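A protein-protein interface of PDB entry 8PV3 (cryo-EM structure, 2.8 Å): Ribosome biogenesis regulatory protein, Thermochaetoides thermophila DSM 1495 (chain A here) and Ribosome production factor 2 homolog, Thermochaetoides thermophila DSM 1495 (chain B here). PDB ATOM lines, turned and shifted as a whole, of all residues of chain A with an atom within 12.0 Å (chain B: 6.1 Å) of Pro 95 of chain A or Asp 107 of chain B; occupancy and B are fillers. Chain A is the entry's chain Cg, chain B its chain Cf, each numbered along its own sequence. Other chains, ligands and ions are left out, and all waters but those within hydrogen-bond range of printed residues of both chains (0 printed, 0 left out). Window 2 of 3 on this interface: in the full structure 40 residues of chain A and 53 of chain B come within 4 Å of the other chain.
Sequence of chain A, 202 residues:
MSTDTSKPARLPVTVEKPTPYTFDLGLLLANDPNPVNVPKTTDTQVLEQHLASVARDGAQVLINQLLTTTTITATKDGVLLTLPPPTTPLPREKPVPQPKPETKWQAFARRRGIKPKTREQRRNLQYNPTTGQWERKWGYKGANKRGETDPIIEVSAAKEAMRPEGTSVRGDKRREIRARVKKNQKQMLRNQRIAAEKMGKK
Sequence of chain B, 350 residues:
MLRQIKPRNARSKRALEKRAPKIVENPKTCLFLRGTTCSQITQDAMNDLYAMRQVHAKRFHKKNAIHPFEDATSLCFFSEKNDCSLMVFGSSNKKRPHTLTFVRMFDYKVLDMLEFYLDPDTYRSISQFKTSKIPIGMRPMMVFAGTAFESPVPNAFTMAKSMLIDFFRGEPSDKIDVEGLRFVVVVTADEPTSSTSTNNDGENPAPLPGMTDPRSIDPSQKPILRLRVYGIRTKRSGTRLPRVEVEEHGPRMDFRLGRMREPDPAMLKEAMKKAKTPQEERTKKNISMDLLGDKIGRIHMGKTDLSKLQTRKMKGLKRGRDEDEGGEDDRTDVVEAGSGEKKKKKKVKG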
ATOM      1  N   LEU A  90     -20.693  32.249 -16.376  1.00  0.00           N
ATOM      2  CA  LEU A  90     -20.909  32.249 -17.814  1.00  0.00           C
ATOM      3  C   LEU A  90     -21.065  30.815 -18.295  1.00  0.00           C
ATOM      4  O   LEU A  90     -20.422  29.906 -17.758  1.00  0.00           O
ATOM      5  CB  LEU A  90     -19.746  32.922 -18.561  1.00  0.00           C
ATOM      6  CG  LEU A  90     -19.664  34.445 -18.453  1.00  0.00           C
ATOM      7  CD1 LEU A  90     -18.308  34.940 -18.918  1.00  0.00           C
ATOM      8  CD2 LEU A  90     -20.776  35.098 -19.250  1.00  0.00           C
ATOM      9  N   PRO A  91     -21.911  30.581 -19.298  1.00  0.00           N
ATOM     10  CA  PRO A  91     -22.124  29.209 -19.770  1.00  0.00           C
ATOM     11  C   PRO A  91     -20.931  28.683 -20.551  1.00  0.00           C
ATOM     12  O   PRO A  91     -20.186  29.441 -21.174  1.00  0.00           O
ATOM     13  CB  PRO A  91     -23.362  29.332 -20.664  1.00  0.00           C
ATOM     14  CG  PRO A  91     -23.330  30.733 -21.136  1.00  0.00           C
ATOM     15  CD  PRO A  91     -22.784  31.540 -19.997  1.00  0.00           C
ATOM     16  N   ARG A  92     -20.760  27.365 -20.510  1.00  0.00           N
ATOM     17  CA  ARG A  92     -19.733  26.705 -21.295  1.00  0.00           C
ATOM     18  C   ARG A  92     -20.229  26.468 -22.718  1.00  0.00           C
ATOM     19  O   ARG A  92     -21.429  26.508 -22.998  1.00  0.00           O
ATOM     20  CB  ARG A  92     -19.336  25.377 -20.649  1.00  0.00           C
ATOM     21  CG  ARG A  92     -18.467  25.522 -19.412  1.00  0.00           C
ATOM     22  CD  ARG A  92     -18.252  24.185 -18.725  1.00  0.00           C
ATOM     23  NE  ARG A  92     -17.653  23.192 -19.609  1.00  0.00           N
ATOM     24  CZ  ARG A  92     -16.356  22.923 -19.661  1.00  0.00           C
ATOM     25  NH1 ARG A  92     -15.490  23.541 -18.875  1.00  0.00           N
ATOM     26  NH2 ARG A  92     -15.917  22.007 -20.519  1.00  0.00           N
ATOM     27  N   GLU A  93     -19.286  26.226 -23.626  1.00  0.00           N
ATOM     28  CA  GLU A  93     -19.651  25.908 -25.000  1.00  0.00           C
ATOM     29  C   GLU A  93     -19.782  24.412 -25.235  1.00  0.00           C
ATOM     30  O   GLU A  93     -20.527  23.993 -26.126  1.00  0.00           O
ATOM     31  CB  GLU A  93     -18.624  26.482 -25.979  1.00  0.00           C
ATOM     32  CG  GLU A  93     -17.191  26.067 -25.703  1.00  0.00           C
ATOM     33  CD  GLU A  93     -16.223  26.587 -26.744  1.00  0.00           C
ATOM     34  OE1 GLU A  93     -16.686  27.115 -27.776  1.00  0.00           O
ATOM     35  OE2 GLU A  93     -14.999  26.457 -26.538  1.00  0.00           O
ATOM     36  N   LYS A  94     -19.071  23.602 -24.459  1.00  0.00           N
ATOM     37  CA  LYS A  94     -19.070  22.156 -24.578  1.00  0.00           C
ATOM     38  C   LYS A  94     -19.203  21.537 -23.196  1.00  0.00           C
ATOM     39  O   LYS A  94     -18.823  22.159 -22.199  1.00  0.00           O
ATOM     40  CB  LYS A  94     -17.781  21.669 -25.259  1.00  0.00           C
ATOM     41  CG  LYS A  94     -17.707  22.027 -26.736  1.00  0.00           C
ATOM     42  CD  LYS A  94     -16.310  21.864 -27.295  1.00  0.00           C
ATOM     43  CE  LYS A  94     -16.231  22.410 -28.709  1.00  0.00           C
ATOM     44  NZ  LYS A  94     -14.840  22.394 -29.236  1.00  0.00           N
ATOM     45  N   PRO A  95     -19.761  20.328 -23.100  1.00  0.00           N
ATOM     46  CA  PRO A  95     -19.927  19.700 -21.784  1.00  0.00           C
ATOM     47  C   PRO A  95     -18.596  19.336 -21.147  1.00  0.00           C
ATOM     48  O   PRO A  95     -17.571  19.208 -21.821  1.00  0.00           O
ATOM     49  CB  PRO A  95     -20.758  18.445 -22.088  1.00  0.00           C
ATOM     50  CG  PRO A  95     -20.603  18.219 -23.549  1.00  0.00           C
ATOM     51  CD  PRO A  95     -20.463  19.573 -24.151  1.00  0.00           C
ATOM     52  N   VAL A  96     -18.624  19.204 -19.822  1.00  0.00           N
ATOM     53  CA  VAL A  96     -17.447  18.792 -19.050  1.00  0.00           C
ATOM     54  C   VAL A  96     -17.036  17.394 -19.491  1.00  0.00           C
ATOM     55  O   VAL A  96     -17.916  16.537 -19.712  1.00  0.00           O
ATOM     56  CB  VAL A  96     -17.761  18.834 -17.543  1.00  0.00           C
ATOM     57  CG1 VAL A  96     -16.642  18.225 -16.712  1.00  0.00           C
ATOM     58  CG2 VAL A  96     -18.038  20.260 -17.103  1.00  0.00           C
ATOM     59  N   PRO A  97     -15.745  17.121 -19.698  1.00  0.00           N
ATOM     60  CA  PRO A  97     -15.322  15.778 -20.117  1.00  0.00           C
ATOM     61  C   PRO A  97     -15.685  14.717 -19.088  1.00  0.00           C
ATOM     62  O   PRO A  97     -15.584  14.935 -17.879  1.00  0.00           O
ATOM     63  CB  PRO A  97     -13.803  15.917 -20.268  1.00  0.00           C
ATOM     64  CG  PRO A  97     -13.583  17.358 -20.529  1.00  0.00           C
ATOM     65  CD  PRO A  97     -14.632  18.087 -19.746  1.00  0.00           C
ATOM     66  N   GLN A  98     -16.107  13.562 -19.584  1.00  0.00           N
ATOM     67  CA  GLN A  98     -16.547  12.439 -18.777  1.00  0.00           C
ATOM     68  C   GLN A  98     -15.690  11.222 -19.091  1.00  0.00           C
ATOM     69  O   GLN A  98     -15.135  11.115 -20.192  1.00  0.00           O
ATOM     70  CB  GLN A  98     -18.026  12.121 -19.046  1.00  0.00           C
ATOM     71  CG  GLN A  98     -19.050  13.187 -18.612  1.00  0.00           C
ATOM     72  CD  GLN A  98     -19.195  13.366 -17.099  1.00  0.00           C
ATOM     73  OE1 GLN A  98     -18.230  13.614 -16.376  1.00  0.00           O
ATOM     74  NE2 GLN A  98     -20.427  13.236 -16.620  1.00  0.00           N
ATOM     75  N   PRO A  99     -15.524  10.307 -18.135  1.00  0.00           N
ATOM     76  CA  PRO A  99     -14.784   9.071 -18.421  1.00  0.00           C
ATOM     77  C   PRO A  99     -15.481   8.236 -19.484  1.00  0.00           C
ATOM     78  O   PRO A  99     -16.710   8.158 -19.536  1.00  0.00           O
ATOM     79  CB  PRO A  99     -14.762   8.353 -17.069  1.00  0.00           C
ATOM     80  CG  PRO A  99     -14.909   9.440 -16.065  1.00  0.00           C
ATOM     81  CD  PRO A  99     -15.822  10.447 -16.699  1.00  0.00           C
ATOM     82  N   PRO B  21     -14.035  18.480 -26.304  1.00  0.00           N
ATOM     83  CA  PRO B  21     -14.282  19.186 -25.038  1.00  0.00           C
ATOM     84  C   PRO B  21     -13.112  19.050 -24.075  1.00  0.00           C
ATOM     85  O   PRO B  21     -12.457  18.008 -24.005  1.00  0.00           O
ATOM     86  CB  PRO B  21     -15.539  18.501 -24.492  1.00  0.00           C
ATOM     87  CG  PRO B  21     -16.209  17.937 -25.692  1.00  0.00           C
ATOM     88  CD  PRO B  21     -15.099  17.506 -26.600  1.00  0.00           C
ATOM     89  N   LYS B  22     -12.859  20.118 -23.321  1.00  0.00           N
ATOM     90  CA  LYS B  22     -11.729  20.176 -22.407  1.00  0.00           C
ATOM     91  C   LYS B  22     -12.203  20.655 -21.043  1.00  0.00           C
ATOM     92  O   LYS B  22     -13.299  21.201 -20.899  1.00  0.00           O
ATOM     93  CB  LYS B  22     -10.623  21.104 -22.927  1.00  0.00           C
ATOM     94  CG  LYS B  22     -10.063  20.719 -24.285  1.00  0.00           C
ATOM     95  CD  LYS B  22      -9.234  21.840 -24.879  1.00  0.00           C
ATOM     96  CE  LYS B  22      -8.765  21.487 -26.277  1.00  0.00           C
ATOM     97  NZ  LYS B  22      -8.022  22.610 -26.911  1.00  0.00           N
ATOM     98  N   GLU B  25     -11.750  25.398 -21.240  1.00  0.00           N
ATOM     99  CA  GLU B  25     -12.222  25.555 -22.605  1.00  0.00           C
ATOM    100  C   GLU B  25     -11.386  26.576 -23.370  1.00  0.00           C
ATOM    101  O   GLU B  25     -10.737  27.454 -22.795  1.00  0.00           O
ATOM    102  CB  GLU B  25     -13.690  25.979 -22.618  1.00  0.00           C
ATOM    103  CG  GLU B  25     -14.659  24.865 -22.278  1.00  0.00           C
ATOM    104  CD  GLU B  25     -16.102  25.304 -22.391  1.00  0.00           C
ATOM    105  OE1 GLU B  25     -16.382  26.497 -22.146  1.00  0.00           O
ATOM    106  OE2 GLU B  25     -16.954  24.458 -22.736  1.00  0.00           O
ATOM    107  N   MET B 105     -24.599  29.114 -28.203  1.00  0.00           N
ATOM    108  CA  MET B 105     -24.705  27.701 -28.514  1.00  0.00           C
ATOM    109  C   MET B 105     -24.143  26.889 -27.356  1.00  0.00           C
ATOM    110  O   MET B 105     -23.257  27.349 -26.631  1.00  0.00           O
ATOM    111  CB  MET B 105     -23.909  27.377 -29.782  1.00  0.00           C
ATOM    112  CG  MET B 105     -24.427  28.028 -31.058  1.00  0.00           C
ATOM    113  SD  MET B 105     -26.094  27.603 -31.582  1.00  0.00           S
ATOM    114  CE  MET B 105     -25.859  25.900 -32.072  1.00  0.00           C
ATOM    115  N   PHE B 106     -24.658  25.673 -27.184  1.00  0.00           N
ATOM    116  CA  PHE B 106     -24.073  24.722 -26.248  1.00  0.00           C
ATOM    117  C   PHE B 106     -24.145  23.322 -26.828  1.00  0.00           C
ATOM    118  O   PHE B 106     -25.231  22.860 -27.189  1.00  0.00           O
ATOM    119  CB  PHE B 106     -24.771  24.747 -24.887  1.00  0.00           C
ATOM    120  CG  PHE B 106     -24.298  23.670 -23.953  1.00  0.00           C
ATOM    121  CD1 PHE B 106     -23.045  23.739 -23.372  1.00  0.00           C
ATOM    122  CD2 PHE B 106     -25.105  22.582 -23.663  1.00  0.00           C
ATOM    123  CE1 PHE B 106     -22.606  22.748 -22.516  1.00  0.00           C
ATOM    124  CE2 PHE B 106     -24.672  21.587 -22.809  1.00  0.00           C
ATOM    125  CZ  PHE B 106     -23.422  21.672 -22.235  1.00  0.00           C
ATOM    126  N   ASP B 107     -22.987  22.654 -26.882  1.00  0.00           N
ATOM    127  CA  ASP B 107     -22.849  21.293 -27.409  1.00  0.00           C
ATOM    128  C   ASP B 107     -23.405  21.193 -28.824  1.00  0.00           C
ATOM    129  O   ASP B 107     -24.096  20.232 -29.174  1.00  0.00           O
ATOM    130  CB  ASP B 107     -23.510  20.267 -26.487  1.00  0.00           C
ATOM    131  CG  ASP B 107     -22.899  18.887 -26.616  1.00  0.00           C
ATOM    132  OD1 ASP B 107     -21.869  18.755 -27.308  1.00  0.00           O
ATOM    133  OD2 ASP B 107     -23.447  17.936 -26.023  1.00  0.00           O
ATOM    134  N   TYR B 108     -23.133  22.232 -29.623  1.00  0.00           N
ATOM    135  CA  TYR B 108     -23.583  22.348 -31.013  1.00  0.00           C
ATOM    136  C   TYR B 108     -25.107  22.357 -31.108  1.00  0.00           C
ATOM    137  O   TYR B 108     -25.683  21.967 -32.125  1.00  0.00           O
ATOM    138  CB  TYR B 108     -22.971  21.248 -31.888  1.00  0.00           C
ATOM    139  CG  TYR B 108     -21.459  21.196 -31.818  1.00  0.00           C
ATOM    140  CD1 TYR B 108     -20.707  22.353 -31.647  1.00  0.00           C
ATOM    141  CD2 TYR B 108     -20.788  19.984 -31.854  1.00  0.00           C
ATOM    142  CE1 TYR B 108     -19.331  22.303 -31.569  1.00  0.00           C
ATOM    143  CE2 TYR B 108     -19.414  19.924 -31.777  1.00  0.00           C
ATOM    144  CZ  TYR B 108     -18.691  21.087 -31.631  1.00  0.00           C
ATOM    145  OH  TYR B 108     -17.320  21.029 -31.550  1.00  0.00           O
ATOM    146  N   LYS B 109     -25.756  22.805 -30.035  1.00  0.00           N
ATOM    147  CA  LYS B 109     -27.198  22.967 -29.964  1.00  0.00           C
ATOM    148  C   LYS B 109     -27.488  24.350 -29.408  1.00  0.00           C
ATOM    149  O   LYS B 109     -26.697  24.900 -28.640  1.00  0.00           O
ATOM    150  CB  LYS B 109     -27.854  21.896 -29.080  1.00  0.00           C
ATOM    151  CG  LYS B 109     -27.672  20.474 -29.580  1.00  0.00           C
ATOM    152  CD  LYS B 109     -28.471  20.236 -30.845  1.00  0.00           C
ATOM    153  CE  LYS B 109     -28.377  18.787 -31.297  1.00  0.00           C
ATOM    154  NZ  LYS B 109     -27.010  18.452 -31.784  1.00  0.00           N
ATOM    155  N   MET B 267     -30.478  21.619 -19.833  1.00  0.00           N
ATOM    156  CA  MET B 267     -29.370  22.055 -20.677  1.00  0.00           C
ATOM    157  C   MET B 267     -28.627  23.220 -20.039  1.00  0.00           C
ATOM    158  O   MET B 267     -27.394  23.291 -20.101  1.00  0.00           O
ATOM    159  CB  MET B 267     -29.895  22.430 -22.064  1.00  0.00           C
ATOM    160  CG  MET B 267     -28.927  23.220 -22.929  1.00  0.00           C
ATOM    161  SD  MET B 267     -29.547  23.504 -24.598  1.00  0.00           S
ATOM    162  CE  MET B 267     -29.155  21.939 -25.373  1.00  0.00           C
ATOM    163  N   GLU B 270     -26.462  21.771 -17.216  1.00  0.00           N
ATOM    164  CA  GLU B 270     -25.289  21.108 -17.776  1.00  0.00           C
ATOM    165  C   GLU B 270     -24.276  22.108 -18.321  1.00  0.00           C
ATOM    166  O   GLU B 270     -23.067  21.921 -18.144  1.00  0.00           O
ATOM    167  CB  GLU B 270     -25.716  20.129 -18.872  1.00  0.00           C
ATOM    168  CG  GLU B 270     -24.582  19.341 -19.529  1.00  0.00           C
ATOM    169  CD  GLU B 270     -23.604  18.722 -18.538  1.00  0.00           C
ATOM    170  OE1 GLU B 270     -22.385  18.767 -18.808  1.00  0.00           O
ATOM    171  OE2 GLU B 270     -24.047  18.153 -17.516  1.00  0.00           O
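O of Lys 22 of chain B sits at hydrogen-bond distance from NH2 of Arg 92 of chain A (2.8 Å). OE2 of Glu 25 of chain B lies within salt-bridge range of NE of Arg 92 of chain A, 3.4 Å away. The side-chain carboxylate (OE2) of Glu 25 of chain B lies within hydrogen-bond range of the backbone NH (N) of Glu 93 of chain A, 3.1 Å away. N of Lys 94 of chain A is in hydrogen-bond range of OE2 of Glu 25 of chain B (2.9 Å). N of Asp 107 of chain B lies within hydrogen-bond range of O of Glu 93 of chain A (2.9 Å).
The backbone carbonyl oxygen (O) of Lys 94 of chain A is in hydrogen-bond range of the guanidinium group (NE) of Arg 92 of chain A (3.0 Å).
CA of Phe 106 of chain B touches O of Glu 93 of chain A (3.6 Å). C of Lys 94 of chain A touches CE1 of Phe 106 of chain B (3.7 Å). Lys 94 of chain A touches Tyr 108 of chain B (CE to OH, 3.3 Å). Pro 21 of chain B touches Pro 95 of chain A. CE1 of Phe 106 of chain B touches N of Pro 95 of chain A, 3.8 Å away. Asp 107 of chain B touches Pro 95 of chain A. Pro 95 of chain A touches Glu 270 of chain B. Glu 270 of chain B touches Val 96 of chain A. Pro 21 of chain B touches Pro 97 of chain A. CD of Pro 97 of chain A touches O of Lys 22 of chain B (3.6 Å).
Of the printed residues of chain B, Glu 93 of chain A touches Glu 25 (3.1 Å), Phe 106 (3.6 Å) and Asp 107 (2.9 Å). Of the printed residues of chain B, Lys 94 of chain A touches Pro 21, Glu 25, Phe 106 and Tyr 108. Pro 95 of chain A touches just these residues of chain B: Pro 21 (3.4 Å), Phe 106 (3.8 Å), Asp 107 (3.5 Å) and Glu 270 (3.7 Å). Of the printed residues of chain B, Val 96 of chain A touches Glu 270 (3.9 Å). Of the printed residues of chain A, Glu 25 of chain B touches Arg 92, Glu 93 and Lys 94. No residue of chain A comes within 4 Å of Met 105 of chain B. Phe 106 of chain B touches just these residues of chain A: Arg 92 (3.2 Å), Glu 93 (3.6 Å), Lys 94 (3.7 Å) and Pro 95 (3.8 Å). Of chain A, only Glu 93 and Pro 95 come within 4 Å of Asp 107 of chain B. Of the printed residues of chain A, Tyr 108 of chain B touches Lys 94. No residue of chain A comes within 4 Å of Lys 109 of chain B. Of the printed residues of chain A, Glu 270 of chain B touches Pro 95 (3.7 Å) and Val 96 (3.9 Å). The nearest residue of chain B that does not touch Pro 95 of chain A is Lys 22 of chain B (4.8 Å).
Of the 10 printed residues of chain A, 6 touch a printed residue of chain B. Printed residues of chain A that touch a printed residue of chain B: Arg 92, Glu 93, Lys 94, Pro 95, Val 96 and Pro 97. Hydrophobic or aromatic side chains of chain B that line the printed part of chain A: Pro 21, Phe 106 and Tyr 108. Among the printed residues, Asp or Glu carboxylates within 4 Å of a Lys or Arg side-chain nitrogen of the other chain: Arg 92 of chain A with Glu 25 of chain B.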
